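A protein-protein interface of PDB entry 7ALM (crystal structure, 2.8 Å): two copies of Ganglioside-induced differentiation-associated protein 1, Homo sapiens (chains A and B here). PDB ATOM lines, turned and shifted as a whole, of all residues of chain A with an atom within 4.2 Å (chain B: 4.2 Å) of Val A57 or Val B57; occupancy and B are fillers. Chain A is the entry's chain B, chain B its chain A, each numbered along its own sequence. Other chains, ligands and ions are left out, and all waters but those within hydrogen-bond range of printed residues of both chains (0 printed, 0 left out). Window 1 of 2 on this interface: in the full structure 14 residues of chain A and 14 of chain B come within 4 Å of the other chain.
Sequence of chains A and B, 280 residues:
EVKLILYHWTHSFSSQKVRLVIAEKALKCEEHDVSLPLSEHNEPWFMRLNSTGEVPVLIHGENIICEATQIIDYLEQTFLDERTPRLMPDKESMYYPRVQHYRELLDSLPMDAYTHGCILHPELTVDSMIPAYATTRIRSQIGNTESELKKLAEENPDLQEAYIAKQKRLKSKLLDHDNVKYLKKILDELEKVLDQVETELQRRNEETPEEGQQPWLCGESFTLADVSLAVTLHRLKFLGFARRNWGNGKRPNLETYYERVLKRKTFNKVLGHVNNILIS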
ATOM      1  N   ILE A   5     -19.700  13.538  15.298  1.00  0.00           N
ATOM      2  CA  ILE A   5     -21.105  13.580  14.907  1.00  0.00           C
ATOM      3  C   ILE A   5     -21.592  12.165  14.627  1.00  0.00           C
ATOM      4  O   ILE A   5     -20.857  11.340  14.071  1.00  0.00           O
ATOM      5  CB  ILE A   5     -21.323  14.479  13.674  1.00  0.00           C
ATOM      6  CG1 ILE A   5     -20.778  15.884  13.941  1.00  0.00           C
ATOM      7  CG2 ILE A   5     -22.801  14.533  13.318  1.00  0.00           C
ATOM      8  CD1 ILE A   5     -20.771  16.784  12.722  1.00  0.00           C
ATOM      9  N   LEU A   6     -22.839  11.892  15.008  1.00  0.00           N
ATOM     10  CA  LEU A   6     -23.472  10.607  14.748  1.00  0.00           C
ATOM     11  C   LEU A   6     -24.909  10.842  14.310  1.00  0.00           C
ATOM     12  O   LEU A   6     -25.671  11.516  15.012  1.00  0.00           O
ATOM     13  CB  LEU A   6     -23.443   9.704  15.987  1.00  0.00           C
ATOM     14  CG  LEU A   6     -24.160   8.358  15.853  1.00  0.00           C
ATOM     15  CD1 LEU A   6     -23.371   7.394  14.984  1.00  0.00           C
ATOM     16  CD2 LEU A   6     -24.417   7.752  17.219  1.00  0.00           C
ATOM     17  N   TYR A   7     -25.271  10.295  13.154  1.00  0.00           N
ATOM     18  CA  TYR A   7     -26.652  10.242  12.693  1.00  0.00           C
ATOM     19  C   TYR A   7     -27.131   8.802  12.805  1.00  0.00           C
ATOM     20  O   TYR A   7     -26.453   7.880  12.339  1.00  0.00           O
ATOM     21  CB  TYR A   7     -26.780  10.755  11.258  1.00  0.00           C
ATOM     22  CG  TYR A   7     -26.546  12.245  11.124  1.00  0.00           C
ATOM     23  CD1 TYR A   7     -25.266  12.754  10.954  1.00  0.00           C
ATOM     24  CD2 TYR A   7     -27.606  13.143  11.166  1.00  0.00           C
ATOM     25  CE1 TYR A   7     -25.045  14.114  10.829  1.00  0.00           C
ATOM     26  CE2 TYR A   7     -27.395  14.506  11.042  1.00  0.00           C
ATOM     27  CZ  TYR A   7     -26.113  14.985  10.874  1.00  0.00           C
ATOM     28  OH  TYR A   7     -25.896  16.338  10.750  1.00  0.00           O
ATOM     29  N   VAL A  55     -28.636   2.184   8.069  1.00  0.00           N
ATOM     30  CA  VAL A  55     -27.263   2.209   8.557  1.00  0.00           C
ATOM     31  C   VAL A  55     -26.941   3.529   9.267  1.00  0.00           C
ATOM     32  O   VAL A  55     -27.299   4.600   8.779  1.00  0.00           O
ATOM     33  CB  VAL A  55     -26.287   1.974   7.390  1.00  0.00           C
ATOM     34  CG1 VAL A  55     -26.183   3.236   6.525  1.00  0.00           C
ATOM     35  CG2 VAL A  55     -24.930   1.543   7.909  1.00  0.00           C
ATOM     36  N   PRO A  56     -26.273   3.460  10.417  1.00  0.00           N
ATOM     37  CA  PRO A  56     -25.788   4.684  11.067  1.00  0.00           C
ATOM     38  C   PRO A  56     -24.529   5.200  10.380  1.00  0.00           C
ATOM     39  O   PRO A  56     -23.943   4.542   9.521  1.00  0.00           O
ATOM     40  CB  PRO A  56     -25.494   4.234  12.501  1.00  0.00           C
ATOM     41  CG  PRO A  56     -25.133   2.798  12.361  1.00  0.00           C
ATOM     42  CD  PRO A  56     -25.974   2.260  11.223  1.00  0.00           C
ATOM     43  N   VAL A  57     -24.114   6.399  10.777  1.00  0.00           N
ATOM     44  CA  VAL A  57     -22.934   7.023  10.186  1.00  0.00           C
ATOM     45  C   VAL A  57     -22.300   7.955  11.206  1.00  0.00           C
ATOM     46  O   VAL A  57     -22.996   8.686  11.919  1.00  0.00           O
ATOM     47  CB  VAL A  57     -23.277   7.785   8.886  1.00  0.00           C
ATOM     48  CG1 VAL A  57     -24.302   8.876   9.147  1.00  0.00           C
ATOM     49  CG2 VAL A  57     -22.016   8.384   8.280  1.00  0.00           C
ATOM     50  N   LEU A  58     -20.970   7.932  11.261  1.00  0.00           N
ATOM     51  CA  LEU A  58     -20.190   8.795  12.135  1.00  0.00           C
ATOM     52  C   LEU A  58     -19.310   9.703  11.288  1.00  0.00           C
ATOM     53  O   LEU A  58     -18.603   9.230  10.391  1.00  0.00           O
ATOM     54  CB  LEU A  58     -19.319   7.974  13.090  1.00  0.00           C
ATOM     55  CG  LEU A  58     -18.558   8.774  14.151  1.00  0.00           C
ATOM     56  CD1 LEU A  58     -19.294   8.745  15.483  1.00  0.00           C
ATOM     57  CD2 LEU A  58     -17.141   8.253  14.308  1.00  0.00           C
ATOM     58  N   ILE A  64     -15.549   9.636   7.537  1.00  0.00           N
ATOM     59  CA  ILE A  64     -16.959   9.275   7.429  1.00  0.00           C
ATOM     60  C   ILE A  64     -17.033   7.753   7.460  1.00  0.00           C
ATOM     61  O   ILE A  64     -16.569   7.088   6.525  1.00  0.00           O
ATOM     62  CB  ILE A  64     -17.608   9.827   6.152  1.00  0.00           C
ATOM     63  CG1 ILE A  64     -17.652  11.357   6.193  1.00  0.00           C
ATOM     64  CG2 ILE A  64     -19.009   9.257   5.982  1.00  0.00           C
ATOM     65  CD1 ILE A  64     -17.942  12.004   4.848  1.00  0.00           C
ATOM     66  N   ILE A  65     -17.620   7.203   8.522  1.00  0.00           N
ATOM     67  CA  ILE A  65     -17.731   5.764   8.719  1.00  0.00           C
ATOM     68  C   ILE A  65     -19.206   5.420   8.889  1.00  0.00           C
ATOM     69  O   ILE A  65     -19.929   6.106   9.620  1.00  0.00           O
ATOM     70  CB  ILE A  65     -16.907   5.298   9.937  1.00  0.00           C
ATOM     71  CG1 ILE A  65     -15.491   5.899   9.905  1.00  0.00           C
ATOM     72  CG2 ILE A  65     -16.809   3.777   9.976  1.00  0.00           C
ATOM     73  CD1 ILE A  65     -15.374   7.273  10.550  1.00  0.00           C
ATOM     74  N   CYS A  66     -19.652   4.356   8.216  1.00  0.00           N
ATOM     75  CA  CYS A  66     -21.082   4.065   8.144  1.00  0.00           C
ATOM     76  C   CYS A  66     -21.496   2.905   9.045  1.00  0.00           C
ATOM     77  O   CYS A  66     -21.959   3.139  10.165  1.00  0.00           O
ATOM     78  CB  CYS A  66     -21.491   3.796   6.687  1.00  0.00           C
ATOM     79  SG  CYS A  66     -21.387   5.285   5.631  1.00  0.00           S
ATOM     80  N   ILE A  71     -18.030   1.691  12.656  1.00  0.00           N
ATOM     81  CA  ILE A  71     -17.969   2.846  13.547  1.00  0.00           C
ATOM     82  C   ILE A  71     -17.240   2.475  14.831  1.00  0.00           C
ATOM     83  O   ILE A  71     -16.340   3.187  15.287  1.00  0.00           O
ATOM     84  CB  ILE A  71     -19.383   3.382  13.842  1.00  0.00           C
ATOM     85  CG1 ILE A  71     -19.946   4.099  12.612  1.00  0.00           C
ATOM     86  CG2 ILE A  71     -19.350   4.300  15.065  1.00  0.00           C
ATOM     87  CD1 ILE A  71     -21.376   4.584  12.772  1.00  0.00           C
ATOM     88  N   ILE B   5     -28.826  16.893   3.645  1.00  0.00           N
ATOM     89  CA  ILE B   5     -27.493  17.061   4.210  1.00  0.00           C
ATOM     90  C   ILE B   5     -26.560  16.066   3.534  1.00  0.00           C
ATOM     91  O   ILE B   5     -26.896  14.885   3.403  1.00  0.00           O
ATOM     92  CB  ILE B   5     -27.486  16.862   5.736  1.00  0.00           C
ATOM     93  CG1 ILE B   5     -28.538  17.755   6.394  1.00  0.00           C
ATOM     94  CG2 ILE B   5     -26.103  17.169   6.291  1.00  0.00           C
ATOM     95  CD1 ILE B   5     -28.695  17.532   7.886  1.00  0.00           C
ATOM     96  N   LEU B   6     -25.390  16.545   3.115  1.00  0.00           N
ATOM     97  CA  LEU B   6     -24.390  15.716   2.459  1.00  0.00           C
ATOM     98  C   LEU B   6     -23.029  15.968   3.088  1.00  0.00           C
ATOM     99  O   LEU B   6     -22.599  17.121   3.206  1.00  0.00           O
ATOM    100  CB  LEU B   6     -24.326  16.004   0.954  1.00  0.00           C
ATOM    101  CG  LEU B   6     -23.230  15.271   0.178  1.00  0.00           C
ATOM    102  CD1 LEU B   6     -23.551  13.788   0.066  1.00  0.00           C
ATOM    103  CD2 LEU B   6     -23.031  15.883  -1.201  1.00  0.00           C
ATOM    104  N   TYR B   7     -22.356  14.891   3.481  1.00  0.00           N
ATOM    105  CA  TYR B   7     -20.967  14.929   3.919  1.00  0.00           C
ATOM    106  C   TYR B   7     -20.118  14.222   2.869  1.00  0.00           C
ATOM    107  O   TYR B   7     -20.448  13.109   2.448  1.00  0.00           O
ATOM    108  CB  TYR B   7     -20.806  14.269   5.288  1.00  0.00           C
ATOM    109  CG  TYR B   7     -21.474  15.028   6.412  1.00  0.00           C
ATOM    110  CD1 TYR B   7     -20.795  16.020   7.104  1.00  0.00           C
ATOM    111  CD2 TYR B   7     -22.784  14.750   6.783  1.00  0.00           C
ATOM    112  CE1 TYR B   7     -21.400  16.715   8.135  1.00  0.00           C
ATOM    113  CE2 TYR B   7     -23.397  15.441   7.813  1.00  0.00           C
ATOM    114  CZ  TYR B   7     -22.699  16.422   8.485  1.00  0.00           C
ATOM    115  OH  TYR B   7     -23.300  17.114   9.513  1.00  0.00           O
ATOM    116  N   VAL B  55     -16.295   6.990   2.002  1.00  0.00           N
ATOM    117  CA  VAL B  55     -17.541   7.083   1.252  1.00  0.00           C
ATOM    118  C   VAL B  55     -18.356   8.299   1.691  1.00  0.00           C
ATOM    119  O   VAL B  55     -18.335   8.670   2.863  1.00  0.00           O
ATOM    120  CB  VAL B  55     -18.370   5.802   1.423  1.00  0.00           C
ATOM    121  CG1 VAL B  55     -17.515   4.578   1.133  1.00  0.00           C
ATOM    122  CG2 VAL B  55     -18.952   5.740   2.829  1.00  0.00           C
ATOM    123  N   PRO B  56     -19.070   8.923   0.757  1.00  0.00           N
ATOM    124  CA  PRO B  56     -19.977  10.014   1.128  1.00  0.00           C
ATOM    125  C   PRO B  56     -21.272   9.483   1.724  1.00  0.00           C
ATOM    126  O   PRO B  56     -21.633   8.315   1.566  1.00  0.00           O
ATOM    127  CB  PRO B  56     -20.233  10.730  -0.202  1.00  0.00           C
ATOM    128  CG  PRO B  56     -20.093   9.654  -1.227  1.00  0.00           C
ATOM    129  CD  PRO B  56     -19.042   8.700  -0.703  1.00  0.00           C
ATOM    130  N   VAL B  57     -21.977  10.372   2.420  1.00  0.00           N
ATOM    131  CA  VAL B  57     -23.220  10.013   3.093  1.00  0.00           C
ATOM    132  C   VAL B  57     -24.225  11.147   2.948  1.00  0.00           C
ATOM    133  O   VAL B  57     -23.870  12.328   3.045  1.00  0.00           O
ATOM    134  CB  VAL B  57     -22.994   9.684   4.583  1.00  0.00           C
ATOM    135  CG1 VAL B  57     -22.423  10.884   5.320  1.00  0.00           C
ATOM    136  CG2 VAL B  57     -24.297   9.244   5.223  1.00  0.00           C
ATOM    137  N   LEU B  58     -25.488  10.777   2.728  1.00  0.00           N
ATOM    138  CA  LEU B  58     -26.597  11.717   2.633  1.00  0.00           C
ATOM    139  C   LEU B  58     -27.585  11.454   3.759  1.00  0.00           C
ATOM    140  O   LEU B  58     -27.944  10.298   4.017  1.00  0.00           O
ATOM    141  CB  LEU B  58     -27.315  11.604   1.285  1.00  0.00           C
ATOM    142  CG  LEU B  58     -28.492  12.562   1.073  1.00  0.00           C
ATOM    143  CD1 LEU B  58     -27.994  13.919   0.594  1.00  0.00           C
ATOM    144  CD2 LEU B  58     -29.509  11.986   0.099  1.00  0.00           C
ATOM    145  N   ILE B  64     -30.732   7.642   5.848  1.00  0.00           N
ATOM    146  CA  ILE B  64     -29.282   7.792   5.821  1.00  0.00           C
ATOM    147  C   ILE B  64     -28.752   6.841   4.756  1.00  0.00           C
ATOM    148  O   ILE B  64     -28.919   5.621   4.874  1.00  0.00           O
ATOM    149  CB  ILE B  64     -28.644   7.483   7.186  1.00  0.00           C
ATOM    150  CG1 ILE B  64     -29.105   8.495   8.235  1.00  0.00           C
ATOM    151  CG2 ILE B  64     -27.128   7.487   7.069  1.00  0.00           C
ATOM    152  CD1 ILE B  64     -28.900   8.033   9.664  1.00  0.00           C
ATOM    153  N   ILE B  65     -28.122   7.390   3.723  1.00  0.00           N
ATOM    154  CA  ILE B  65     -27.660   6.606   2.584  1.00  0.00           C
ATOM    155  C   ILE B  65     -26.168   6.857   2.396  1.00  0.00           C
ATOM    156  O   ILE B  65     -25.739   8.011   2.262  1.00  0.00           O
ATOM    157  CB  ILE B  65     -28.436   6.948   1.303  1.00  0.00           C
ATOM    158  CG1 ILE B  65     -29.947   6.914   1.550  1.00  0.00           C
ATOM    159  CG2 ILE B  65     -28.084   5.972   0.192  1.00  0.00           C
ATOM    160  CD1 ILE B  65     -30.529   8.241   1.991  1.00  0.00           C
ATOM    161  N   CYS B  66     -25.385   5.780   2.389  1.00  0.00           N
ATOM    162  CA  CYS B  66     -23.955   5.836   2.124  1.00  0.00           C
ATOM    163  C   CYS B  66     -23.658   5.348   0.707  1.00  0.00           C
ATOM    164  O   CYS B  66     -24.494   4.730   0.044  1.00  0.00           O
ATOM    165  CB  CYS B  66     -23.178   5.000   3.151  1.00  0.00           C
ATOM    166  SG  CYS B  66     -23.243   5.634   4.854  1.00  0.00           S
ATOM    167  N   ILE B  71     -26.678   6.747  -3.088  1.00  0.00           N
ATOM    168  CA  ILE B  71     -27.188   8.102  -2.896  1.00  0.00           C
ATOM    169  C   ILE B  71     -27.923   8.574  -4.144  1.00  0.00           C
ATOM    170  O   ILE B  71     -29.021   9.136  -4.066  1.00  0.00           O
ATOM    171  CB  ILE B  71     -26.042   9.063  -2.534  1.00  0.00           C
ATOM    172  CG1 ILE B  71     -25.553   8.803  -1.110  1.00  0.00           C
ATOM    173  CG2 ILE B  71     -26.494  10.510  -2.707  1.00  0.00           C
ATOM    174  CD1 ILE B  71     -24.262   9.521  -0.772  1.00  0.00           C
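Among the printed residues, pairs that only touch across the chains: Ile A64 with Val B55 (3.2 Å), Val A55 with Ile B64 (3.4 Å), Tyr A7 with Ile B64 (3.6 Å), Ile A64 with Tyr B7 (3.6 Å), Cys A66 with Val B55 (3.7 Å), Val A57 with Ile B64 (3.8 Å), Ile A64 with Val B57 (3.8 Å) and Val A57 with Val B57 (3.9 Å).
The side-chain sulfur of Cys B66 is disulfide-bonded to the side-chain sulfur of Cys A66 (2.0 Å). OH of Tyr A7 sits at hydrogen-bond distance from OH of Tyr B7 (3.0 Å).
The backbone carbonyl oxygen of Pro A56 sits close to the backbone carbonyl oxygen of Cys A66, at 2.5 Å. N of Tyr B7 lies within hydrogen-bond range of O of Val B57, at 3.0 Å. O of Val A57 is in hydrogen-bond range of N of Tyr A7 (3.0 Å).
Val B57 touches just these residues of chain A: Val A57 and Ile A64. Printed residues of chain A within 4 Å of Tyr B7: Tyr A7 (3.0 Å) and Ile A64 (3.6 Å). Printed residues of chain A within 4 Å of Ile B64: Tyr A7, Val A55 and Val A57. Of the printed residues of chain B, Tyr A7 touches Tyr B7 (3.0 Å) and Ile B64 (3.6 Å). The nearest printed residue of chain B that does not touch Val A57 is Cys B66 (4.6 Å). The nearest printed residue of chain B that does not touch Ile A64 is Pro B56 (4.7 Å).
Tyr A7 touches Ile B64, and with the chains exchanged Ile A64 touches Tyr B7. Val A57 touches Ile B64, and with the chains exchanged Ile A64 touches Val B57. Cys A66 touches Val B55, but with the chains exchanged Val A55 does not touch Cys B66 (4.1 Å). Cys A66 touches its own counterpart, Cys B66. 11 positions are printed for both chains. Of the 10 pairs that touch across the chains among the printed residues, 9 have their exchanged pair printed and touching as well.
Hydrophobic or aromatic side chains of chain B within 4 Å of the printed part of chain A: Tyr B7, Val B55, Val B57 and Ile B64. Along chain B the printed residues that touch a printed residue of chain A span positions 7 to 66. Among the printed residues, 10 pairs touch across the chains. Among the printed residues, no Asp or Glu carboxylate lies within 4 Å of a Lys or Arg side-chain nitrogen of the other chain.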
